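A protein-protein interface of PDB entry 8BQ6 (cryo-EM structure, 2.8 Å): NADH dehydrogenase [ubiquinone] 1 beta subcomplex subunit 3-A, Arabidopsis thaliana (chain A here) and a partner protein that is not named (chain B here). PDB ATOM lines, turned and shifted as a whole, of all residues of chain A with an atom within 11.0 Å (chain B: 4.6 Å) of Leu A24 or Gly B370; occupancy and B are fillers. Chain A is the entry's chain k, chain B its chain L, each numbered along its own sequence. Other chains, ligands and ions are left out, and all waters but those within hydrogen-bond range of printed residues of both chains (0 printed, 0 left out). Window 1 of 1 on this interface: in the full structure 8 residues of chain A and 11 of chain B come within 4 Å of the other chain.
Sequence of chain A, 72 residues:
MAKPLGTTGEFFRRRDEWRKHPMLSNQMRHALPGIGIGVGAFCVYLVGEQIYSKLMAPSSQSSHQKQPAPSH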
ATOM      1  N   ASP A  16     -17.691  14.489  -0.899  1.00  0.00           N
ATOM      2  CA  ASP A  16     -18.515  15.121  -1.918  1.00  0.00           C
ATOM      3  C   ASP A  16     -18.713  14.230  -3.121  1.00  0.00           C
ATOM      4  O   ASP A  16     -19.131  14.703  -4.185  1.00  0.00           O
ATOM      5  CB  ASP A  16     -17.888  16.439  -2.353  1.00  0.00           C
ATOM      6  CG  ASP A  16     -18.195  17.556  -1.402  1.00  0.00           C
ATOM      7  OD1 ASP A  16     -19.369  17.671  -0.999  1.00  0.00           O
ATOM      8  OD2 ASP A  16     -17.265  18.304  -1.041  1.00  0.00           O
ATOM      9  N   GLU A  17     -18.408  12.948  -2.974  1.00  0.00           N
ATOM     10  CA  GLU A  17     -18.373  12.063  -4.126  1.00  0.00           C
ATOM     11  C   GLU A  17     -19.778  11.700  -4.592  1.00  0.00           C
ATOM     12  O   GLU A  17     -19.944  11.216  -5.717  1.00  0.00           O
ATOM     13  CB  GLU A  17     -17.483  10.860  -3.772  1.00  0.00           C
ATOM     14  CG  GLU A  17     -16.012  11.164  -3.577  1.00  0.00           C
ATOM     15  CD  GLU A  17     -15.232   9.989  -3.174  1.00  0.00           C
ATOM     16  OE1 GLU A  17     -15.869   8.971  -2.861  1.00  0.00           O
ATOM     17  OE2 GLU A  17     -13.979  10.105  -3.119  1.00  0.00           O
ATOM     18  N   TRP A  18     -20.800  11.958  -3.767  1.00  0.00           N
ATOM     19  CA  TRP A  18     -22.178  11.830  -4.238  1.00  0.00           C
ATOM     20  C   TRP A  18     -22.600  12.994  -5.130  1.00  0.00           C
ATOM     21  O   TRP A  18     -23.593  12.872  -5.855  1.00  0.00           O
ATOM     22  CB  TRP A  18     -23.161  11.720  -3.064  1.00  0.00           C
ATOM     23  CG  TRP A  18     -23.275  12.961  -2.222  1.00  0.00           C
ATOM     24  CD1 TRP A  18     -22.595  13.238  -1.072  1.00  0.00           C
ATOM     25  CD2 TRP A  18     -24.109  14.098  -2.475  1.00  0.00           C
ATOM     26  NE1 TRP A  18     -22.957  14.472  -0.591  1.00  0.00           N
ATOM     27  CE2 TRP A  18     -23.886  15.019  -1.435  1.00  0.00           C
ATOM     28  CE3 TRP A  18     -25.026  14.423  -3.478  1.00  0.00           C
ATOM     29  CZ2 TRP A  18     -24.544  16.243  -1.371  1.00  0.00           C
ATOM     30  CZ3 TRP A  18     -25.675  15.637  -3.413  1.00  0.00           C
ATOM     31  CH2 TRP A  18     -25.433  16.532  -2.369  1.00  0.00           C
ATOM     32  N   ARG A  19     -21.879  14.118  -5.098  1.00  0.00           N
ATOM     33  CA  ARG A  19     -22.267  15.274  -5.904  1.00  0.00           C
ATOM     34  C   ARG A  19     -22.044  15.061  -7.395  1.00  0.00           C
ATOM     35  O   ARG A  19     -22.377  15.950  -8.186  1.00  0.00           O
ATOM     36  CB  ARG A  19     -21.517  16.522  -5.440  1.00  0.00           C
ATOM     37  CG  ARG A  19     -22.153  17.177  -4.230  1.00  0.00           C
ATOM     38  CD  ARG A  19     -21.291  18.273  -3.656  1.00  0.00           C
ATOM     39  NE  ARG A  19     -21.313  18.251  -2.200  1.00  0.00           N
ATOM     40  CZ  ARG A  19     -22.197  18.902  -1.457  1.00  0.00           C
ATOM     41  NH1 ARG A  19     -23.170  19.612  -2.004  1.00  0.00           N
ATOM     42  NH2 ARG A  19     -22.105  18.836  -0.133  1.00  0.00           N
ATOM     43  N   LYS A  20     -21.491  13.919  -7.793  1.00  0.00           N
ATOM     44  CA  LYS A  20     -21.410  13.531  -9.195  1.00  0.00           C
ATOM     45  C   LYS A  20     -22.667  12.827  -9.670  1.00  0.00           C
ATOM     46  O   LYS A  20     -22.611  12.057 -10.636  1.00  0.00           O
ATOM     47  CB  LYS A  20     -20.188  12.640  -9.429  1.00  0.00           C
ATOM     48  CG  LYS A  20     -18.888  13.232  -8.918  1.00  0.00           C
ATOM     49  CD  LYS A  20     -18.767  14.698  -9.306  1.00  0.00           C
ATOM     50  CE  LYS A  20     -17.382  15.237  -9.008  1.00  0.00           C
ATOM     51  NZ  LYS A  20     -16.832  15.996 -10.166  1.00  0.00           N
ATOM     52  N   HIS A  21     -23.784  13.076  -8.999  1.00  0.00           N
ATOM     53  CA  HIS A  21     -25.046  12.456  -9.361  1.00  0.00           C
ATOM     54  C   HIS A  21     -25.363  12.751 -10.826  1.00  0.00           C
ATOM     55  O   HIS A  21     -25.042  13.840 -11.320  1.00  0.00           O
ATOM     56  CB  HIS A  21     -26.156  12.989  -8.452  1.00  0.00           C
ATOM     57  CG  HIS A  21     -27.159  11.959  -8.040  1.00  0.00           C
ATOM     58  ND1 HIS A  21     -28.133  11.483  -8.891  1.00  0.00           N
ATOM     59  CD2 HIS A  21     -27.335  11.310  -6.866  1.00  0.00           C
ATOM     60  CE1 HIS A  21     -28.869  10.589  -8.257  1.00  0.00           C
ATOM     61  NE2 HIS A  21     -28.406  10.465  -7.026  1.00  0.00           N
ATOM     62  N   PRO A  22     -25.935  11.796 -11.561  1.00  0.00           N
ATOM     63  CA  PRO A  22     -26.226  12.051 -12.981  1.00  0.00           C
ATOM     64  C   PRO A  22     -27.076  13.286 -13.223  1.00  0.00           C
ATOM     65  O   PRO A  22     -26.699  14.144 -14.031  1.00  0.00           O
ATOM     66  CB  PRO A  22     -26.945  10.770 -13.418  1.00  0.00           C
ATOM     67  CG  PRO A  22     -26.409   9.721 -12.510  1.00  0.00           C
ATOM     68  CD  PRO A  22     -26.154  10.388 -11.191  1.00  0.00           C
ATOM     69  N   MET A  23     -28.206  13.412 -12.533  1.00  0.00           N
ATOM     70  CA  MET A  23     -29.142  14.501 -12.768  1.00  0.00           C
ATOM     71  C   MET A  23     -28.974  15.652 -11.785  1.00  0.00           C
ATOM     72  O   MET A  23     -29.823  16.547 -11.737  1.00  0.00           O
ATOM     73  CB  MET A  23     -30.575  13.968 -12.740  1.00  0.00           C
ATOM     74  CG  MET A  23     -31.033  13.501 -11.388  1.00  0.00           C
ATOM     75  SD  MET A  23     -32.559  12.560 -11.528  1.00  0.00           S
ATOM     76  CE  MET A  23     -31.908  10.919 -11.809  1.00  0.00           C
ATOM     77  N   LEU A  24     -27.897  15.650 -11.002  1.00  0.00           N
ATOM     78  CA  LEU A  24     -27.523  16.808 -10.209  1.00  0.00           C
ATOM     79  C   LEU A  24     -26.378  17.594 -10.829  1.00  0.00           C
ATOM     80  O   LEU A  24     -26.194  18.767 -10.491  1.00  0.00           O
ATOM     81  CB  LEU A  24     -27.135  16.379  -8.790  1.00  0.00           C
ATOM     82  CG  LEU A  24     -28.265  15.942  -7.858  1.00  0.00           C
ATOM     83  CD1 LEU A  24     -27.845  16.129  -6.410  1.00  0.00           C
ATOM     84  CD2 LEU A  24     -29.559  16.690  -8.151  1.00  0.00           C
ATOM     85  N   SER A  25     -25.612  16.984 -11.725  1.00  0.00           N
ATOM     86  CA  SER A  25     -24.494  17.647 -12.372  1.00  0.00           C
ATOM     87  C   SER A  25     -24.831  17.930 -13.828  1.00  0.00           C
ATOM     88  O   SER A  25     -25.852  17.478 -14.357  1.00  0.00           O
ATOM     89  CB  SER A  25     -23.218  16.803 -12.273  1.00  0.00           C
ATOM     90  OG  SER A  25     -22.807  16.676 -10.924  1.00  0.00           O
ATOM     91  N   ASN A  26     -23.946  18.696 -14.470  1.00  0.00           N
ATOM     92  CA  ASN A  26     -24.105  19.092 -15.869  1.00  0.00           C
ATOM     93  C   ASN A  26     -25.428  19.817 -16.092  1.00  0.00           C
ATOM     94  O   ASN A  26     -26.151  19.550 -17.054  1.00  0.00           O
ATOM     95  CB  ASN A  26     -23.982  17.886 -16.800  1.00  0.00           C
ATOM     96  CG  ASN A  26     -22.701  17.901 -17.602  1.00  0.00           C
ATOM     97  OD1 ASN A  26     -21.698  18.473 -17.177  1.00  0.00           O
ATOM     98  ND2 ASN A  26     -22.725  17.270 -18.770  1.00  0.00           N
ATOM     99  N   GLN A  27     -25.750  20.751 -15.202  1.00  0.00           N
ATOM    100  CA  GLN A  27     -27.043  21.415 -15.265  1.00  0.00           C
ATOM    101  C   GLN A  27     -27.086  22.551 -16.278  1.00  0.00           C
ATOM    102  O   GLN A  27     -28.156  23.135 -16.479  1.00  0.00           O
ATOM    103  CB  GLN A  27     -27.428  21.945 -13.885  1.00  0.00           C
ATOM    104  CG  GLN A  27     -27.725  20.863 -12.865  1.00  0.00           C
ATOM    105  CD  GLN A  27     -28.837  19.935 -13.299  1.00  0.00           C
ATOM    106  OE1 GLN A  27     -29.852  20.374 -13.839  1.00  0.00           O
ATOM    107  NE2 GLN A  27     -28.664  18.646 -13.039  1.00  0.00           N
ATOM    108  N   MET A  28     -25.962  22.885 -16.914  1.00  0.00           N
ATOM    109  CA  MET A  28     -25.973  23.963 -17.894  1.00  0.00           C
ATOM    110  C   MET A  28     -26.618  23.539 -19.206  1.00  0.00           C
ATOM    111  O   MET A  28     -27.019  24.403 -19.993  1.00  0.00           O
ATOM    112  CB  MET A  28     -24.547  24.471 -18.133  1.00  0.00           C
ATOM    113  CG  MET A  28     -24.455  25.813 -18.868  1.00  0.00           C
ATOM    114  SD  MET A  28     -24.847  27.309 -17.922  1.00  0.00           S
ATOM    115  CE  MET A  28     -24.802  26.730 -16.228  1.00  0.00           C
ATOM    116  N   ARG A  29     -26.732  22.235 -19.458  1.00  0.00           N
ATOM    117  CA  ARG A  29     -27.449  21.761 -20.633  1.00  0.00           C
ATOM    118  C   ARG A  29     -28.957  21.822 -20.451  1.00  0.00           C
ATOM    119  O   ARG A  29     -29.693  21.539 -21.403  1.00  0.00           O
ATOM    120  CB  ARG A  29     -27.013  20.338 -20.968  1.00  0.00           C
ATOM    121  CG  ARG A  29     -25.598  20.036 -20.529  1.00  0.00           C
ATOM    122  CD  ARG A  29     -25.440  18.574 -20.195  1.00  0.00           C
ATOM    123  NE  ARG A  29     -26.567  18.072 -19.419  1.00  0.00           N
ATOM    124  CZ  ARG A  29     -26.766  16.792 -19.141  1.00  0.00           C
ATOM    125  NH1 ARG A  29     -25.910  15.860 -19.526  1.00  0.00           N
ATOM    126  NH2 ARG A  29     -27.854  16.437 -18.462  1.00  0.00           N
ATOM    127  N   HIS A  30     -29.430  22.161 -19.255  1.00  0.00           N
ATOM    128  CA  HIS A  30     -30.837  22.420 -19.003  1.00  0.00           C
ATOM    129  C   HIS A  30     -31.131  23.907 -18.865  1.00  0.00           C
ATOM    130  O   HIS A  30     -32.264  24.281 -18.552  1.00  0.00           O
ATOM    131  CB  HIS A  30     -31.289  21.672 -17.747  1.00  0.00           C
ATOM    132  CG  HIS A  30     -31.453  20.199 -17.951  1.00  0.00           C
ATOM    133  ND1 HIS A  30     -30.393  19.318 -17.908  1.00  0.00           N
ATOM    134  CD2 HIS A  30     -32.554  19.449 -18.197  1.00  0.00           C
ATOM    135  CE1 HIS A  30     -30.833  18.091 -18.121  1.00  0.00           C
ATOM    136  NE2 HIS A  30     -32.141  18.143 -18.298  1.00  0.00           N
ATOM    137  N   ALA A  31     -30.135  24.761 -19.120  1.00  0.00           N
ATOM    138  CA  ALA A  31     -30.275  26.191 -18.863  1.00  0.00           C
ATOM    139  C   ALA A  31     -31.385  26.823 -19.689  1.00  0.00           C
ATOM    140  O   ALA A  31     -32.085  27.717 -19.199  1.00  0.00           O
ATOM    141  CB  ALA A  31     -28.952  26.905 -19.135  1.00  0.00           C
ATOM    142  N   GLY B 369     -28.020  24.807  -5.857  1.00  0.00           N
ATOM    143  CA  GLY B 369     -27.310  24.571  -7.095  1.00  0.00           C
ATOM    144  C   GLY B 369     -27.537  23.160  -7.604  1.00  0.00           C
ATOM    145  O   GLY B 369     -27.628  22.196  -6.835  1.00  0.00           O
ATOM    146  N   GLY B 370     -27.602  23.030  -8.925  1.00  0.00           N
ATOM    147  CA  GLY B 370     -27.982  21.757  -9.514  1.00  0.00           C
ATOM    148  C   GLY B 370     -29.434  21.399  -9.287  1.00  0.00           C
ATOM    149  O   GLY B 370     -29.757  20.228  -9.052  1.00  0.00           O
ATOM    150  N   LEU B 371     -30.324  22.390  -9.367  1.00  0.00           N
ATOM    151  CA  LEU B 371     -31.751  22.202  -9.144  1.00  0.00           C
ATOM    152  C   LEU B 371     -32.598  22.417 -10.392  1.00  0.00           C
ATOM    153  O   LEU B 371     -33.826  22.317 -10.308  1.00  0.00           O
ATOM    154  CB  LEU B 371     -32.243  23.144  -8.038  1.00  0.00           C
ATOM    155  CG  LEU B 371     -32.122  22.794  -6.553  1.00  0.00           C
ATOM    156  CD1 LEU B 371     -30.840  22.058  -6.204  1.00  0.00           C
ATOM    157  CD2 LEU B 371     -32.219  24.079  -5.763  1.00  0.00           C
ATOM    158  N   ALA B 372     -31.992  22.719 -11.543  1.00  0.00           N
ATOM    159  CA  ALA B 372     -32.786  22.913 -12.755  1.00  0.00           C
ATOM    160  C   ALA B 372     -33.508  21.632 -13.161  1.00  0.00           C
ATOM    161  O   ALA B 372     -34.704  21.658 -13.475  1.00  0.00           O
ATOM    162  CB  ALA B 372     -31.903  23.413 -13.896  1.00  0.00           C
ATOM    163  N   THR B 441     -28.551  29.187  -7.803  1.00  0.00           N
ATOM    164  CA  THR B 441     -29.659  28.383  -7.307  1.00  0.00           C
ATOM    165  C   THR B 441     -29.848  27.112  -8.122  1.00  0.00           C
ATOM    166  O   THR B 441     -30.070  26.037  -7.555  1.00  0.00           O
ATOM    167  CB  THR B 441     -30.946  29.205  -7.310  1.00  0.00           C
ATOM    168  OG1 THR B 441     -30.717  30.455  -6.648  1.00  0.00           O
ATOM    169  CG2 THR B 441     -32.055  28.453  -6.595  1.00  0.00           C
ATOM    170  N   PHE B 442     -29.796  27.218  -9.451  1.00  0.00           N
ATOM    171  CA  PHE B 442     -30.193  26.037 -10.259  1.00  0.00           C
ATOM    172  C   PHE B 442     -29.151  25.493 -11.233  1.00  0.00           C
ATOM    173  O   PHE B 442     -29.341  24.339 -11.656  1.00  0.00           O
ATOM    174  CB  PHE B 442     -31.358  26.441 -11.163  1.00  0.00           C
ATOM    175  CG  PHE B 442     -32.606  26.952 -10.493  1.00  0.00           C
ATOM    176  CD1 PHE B 442     -33.535  26.075  -9.960  1.00  0.00           C
ATOM    177  CD2 PHE B 442     -32.878  28.310 -10.446  1.00  0.00           C
ATOM    178  CE1 PHE B 442     -34.694  26.546  -9.365  1.00  0.00           C
ATOM    179  CE2 PHE B 442     -34.036  28.781  -9.851  1.00  0.00           C
ATOM    180  CZ  PHE B 442     -34.942  27.897  -9.314  1.00  0.00           C
ATOM    181  N   LEU B 443     -28.080  26.223 -11.543  1.00  0.00           N
ATOM    182  CA  LEU B 443     -27.216  25.801 -12.635  1.00  0.00           C
ATOM    183  C   LEU B 443     -25.823  25.361 -12.216  1.00  0.00           C
ATOM    184  O   LEU B 443     -25.218  24.546 -12.915  1.00  0.00           O
ATOM    185  CB  LEU B 443     -27.094  26.931 -13.661  1.00  0.00           C
ATOM    186  CG  LEU B 443     -28.450  27.301 -14.259  1.00  0.00           C
ATOM    187  CD1 LEU B 443     -28.325  28.345 -15.344  1.00  0.00           C
ATOM    188  CD2 LEU B 443     -29.130  26.055 -14.793  1.00  0.00           C
ATOM    189  N   VAL B 444     -25.292  25.872 -11.110  1.00  0.00           N
ATOM    190  CA  VAL B 444     -23.941  25.508 -10.691  1.00  0.00           C
ATOM    191  C   VAL B 444     -23.961  24.087 -10.136  1.00  0.00           C
ATOM    192  O   VAL B 444     -25.037  23.576  -9.793  1.00  0.00           O
ATOM    193  CB  VAL B 444     -23.384  26.502  -9.658  1.00  0.00           C
ATOM    194  CG1 VAL B 444     -23.168  27.868 -10.296  1.00  0.00           C
ATOM    195  CG2 VAL B 444     -24.299  26.589  -8.448  1.00  0.00           C
ATOM    196  N   PRO B 445     -22.821  23.402 -10.070  1.00  0.00           N
ATOM    197  CA  PRO B 445     -22.787  22.098  -9.394  1.00  0.00           C
ATOM    198  C   PRO B 445     -23.256  22.221  -7.952  1.00  0.00           C
ATOM    199  O   PRO B 445     -22.903  23.169  -7.248  1.00  0.00           O
ATOM    200  CB  PRO B 445     -21.313  21.685  -9.469  1.00  0.00           C
ATOM    201  CG  PRO B 445     -20.667  22.593 -10.457  1.00  0.00           C
ATOM    202  CD  PRO B 445     -21.611  23.668 -10.867  1.00  0.00           C
ATOM    203  N   THR B 446     -24.025  21.225  -7.511  1.00  0.00           N
ATOM    204  CA  THR B 446     -24.759  21.330  -6.257  1.00  0.00           C
ATOM    205  C   THR B 446     -23.843  21.682  -5.098  1.00  0.00           C
ATOM    206  O   THR B 446     -22.776  21.089  -4.918  1.00  0.00           O
ATOM    207  CB  THR B 446     -25.485  20.024  -5.932  1.00  0.00           C
ATOM    208  OG1 THR B 446     -24.613  19.173  -5.180  1.00  0.00           O
ATOM    209  CG2 THR B 446     -25.908  19.317  -7.197  1.00  0.00           C
ATOM    210  N   ILE B 453     -31.809  17.241  -0.685  1.00  0.00           N
ATOM    211  CA  ILE B 453     -31.964  16.794  -2.067  1.00  0.00           C
ATOM    212  C   ILE B 453     -32.845  15.555  -2.135  1.00  0.00           C
ATOM    213  O   ILE B 453     -33.662  15.400  -3.051  1.00  0.00           O
ATOM    214  CB  ILE B 453     -30.581  16.548  -2.697  1.00  0.00           C
ATOM    215  CG1 ILE B 453     -29.949  17.875  -3.115  1.00  0.00           C
ATOM    216  CG2 ILE B 453     -30.678  15.620  -3.891  1.00  0.00           C
ATOM    217  CD1 ILE B 453     -30.870  18.748  -3.924  1.00  0.00           C
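The backbone carbonyl oxygen (O) of Thr B446 is in hydrogen-bond range of the guanidinium group (NH1) of Arg A19.
The backbone carbonyl oxygen (O) of Phe B442 is in hydrogen-bond range of the backbone NH (N) of Gly B370, 3.5 Å away. O of Val B444 is in hydrogen-bond range of N of Gly B370, 2.8 Å away. N of Leu B371 sits at hydrogen-bond distance from O of Phe B442 (3.2 Å). The backbone NH (N) of Ala B372 sits at hydrogen-bond distance from the backbone carbonyl oxygen (O) of Phe B442, 3.1 Å away. NH2 of Arg A19 lies within salt-bridge range of OD1 of Asp A16. The side-chain amide nitrogen (NE2) of Gln A27 is in hydrogen-bond range of the backbone carbonyl oxygen (O) of Ser A25 (3.3 Å).
OG1 of Thr B446 touches CH2 of Trp A18 (3.9 Å). CA of Gly B370 touches O of Leu A24, 3.6 Å away. CG2 of Thr B446 touches O of Leu A24 (3.4 Å). Leu A24 touches Ile B453 (CD1 to CG2, 3.8 Å). CG of Gln A27 touches CA of Gly B370, at 3.5 Å. CB of Ala B372 touches OE1 of Gln A27, at 3.7 Å. Gln A27 touches Phe B442 (CB to O, 3.8 Å). O of Gln A27 touches CD2 of Leu B443 (3.5 Å). Met A28 touches Leu B443 (CE to CB, 3.4 Å).
Of the printed residues of chain B, Trp A18 touches Thr B446. Leu A24 touches just these residues of chain B: Gly B370 (3.6 Å), Thr B446 (3.4 Å) and Ile B453 (3.8 Å). Printed residues of chain B within 4 Å of Gln A27: Gly B370, Ala B372, Phe B442 and Leu B443. Of the printed residues of chain B, Met A28 touches Leu B443 (3.4 Å). No residue of chain A comes within 4 Å of Gly B369. Gly B370 touches just these residues of chain A: Leu A24 and Gln A27. No residue of chain A comes within 4 Å of Leu B371. Of the printed residues of chain A, Ala B372 touches Gln A27. Of the printed residues of chain A, Leu B443 touches Gln A27 (3.5 Å) and Met A28 (3.4 Å). Val B444 touches none of the printed residues of chain A. No residue of chain A comes within 4 Å of Pro B445. Thr B446 touches just these residues of chain A: Trp A18, Arg A19 and Leu A24. Printed residues of chain A within 4 Å of Ile B453: Leu A24 (3.8 Å). The nearest printed residue of chain B that does not touch Arg A19 is Pro B445 (6.0 Å).
Of the 16 printed residues of chain A, 5 touch a printed residue of chain B. Printed residues of chain A that touch a printed residue of chain B: Trp A18, Arg A19, Leu A24, Gln A27 and Met A28. Hydrophobic or aromatic side chains of chain A within 4 Å of the printed part of chain B: Trp A18, Leu A24 and Met A28. Of the 11 printed residues of chain B, 6 touch a printed residue of chain A. Printed residues of chain B that touch a printed residue of chain A: Gly B370, Ala B372, Phe B442, Leu B443, Thr B446 and Ile B453.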
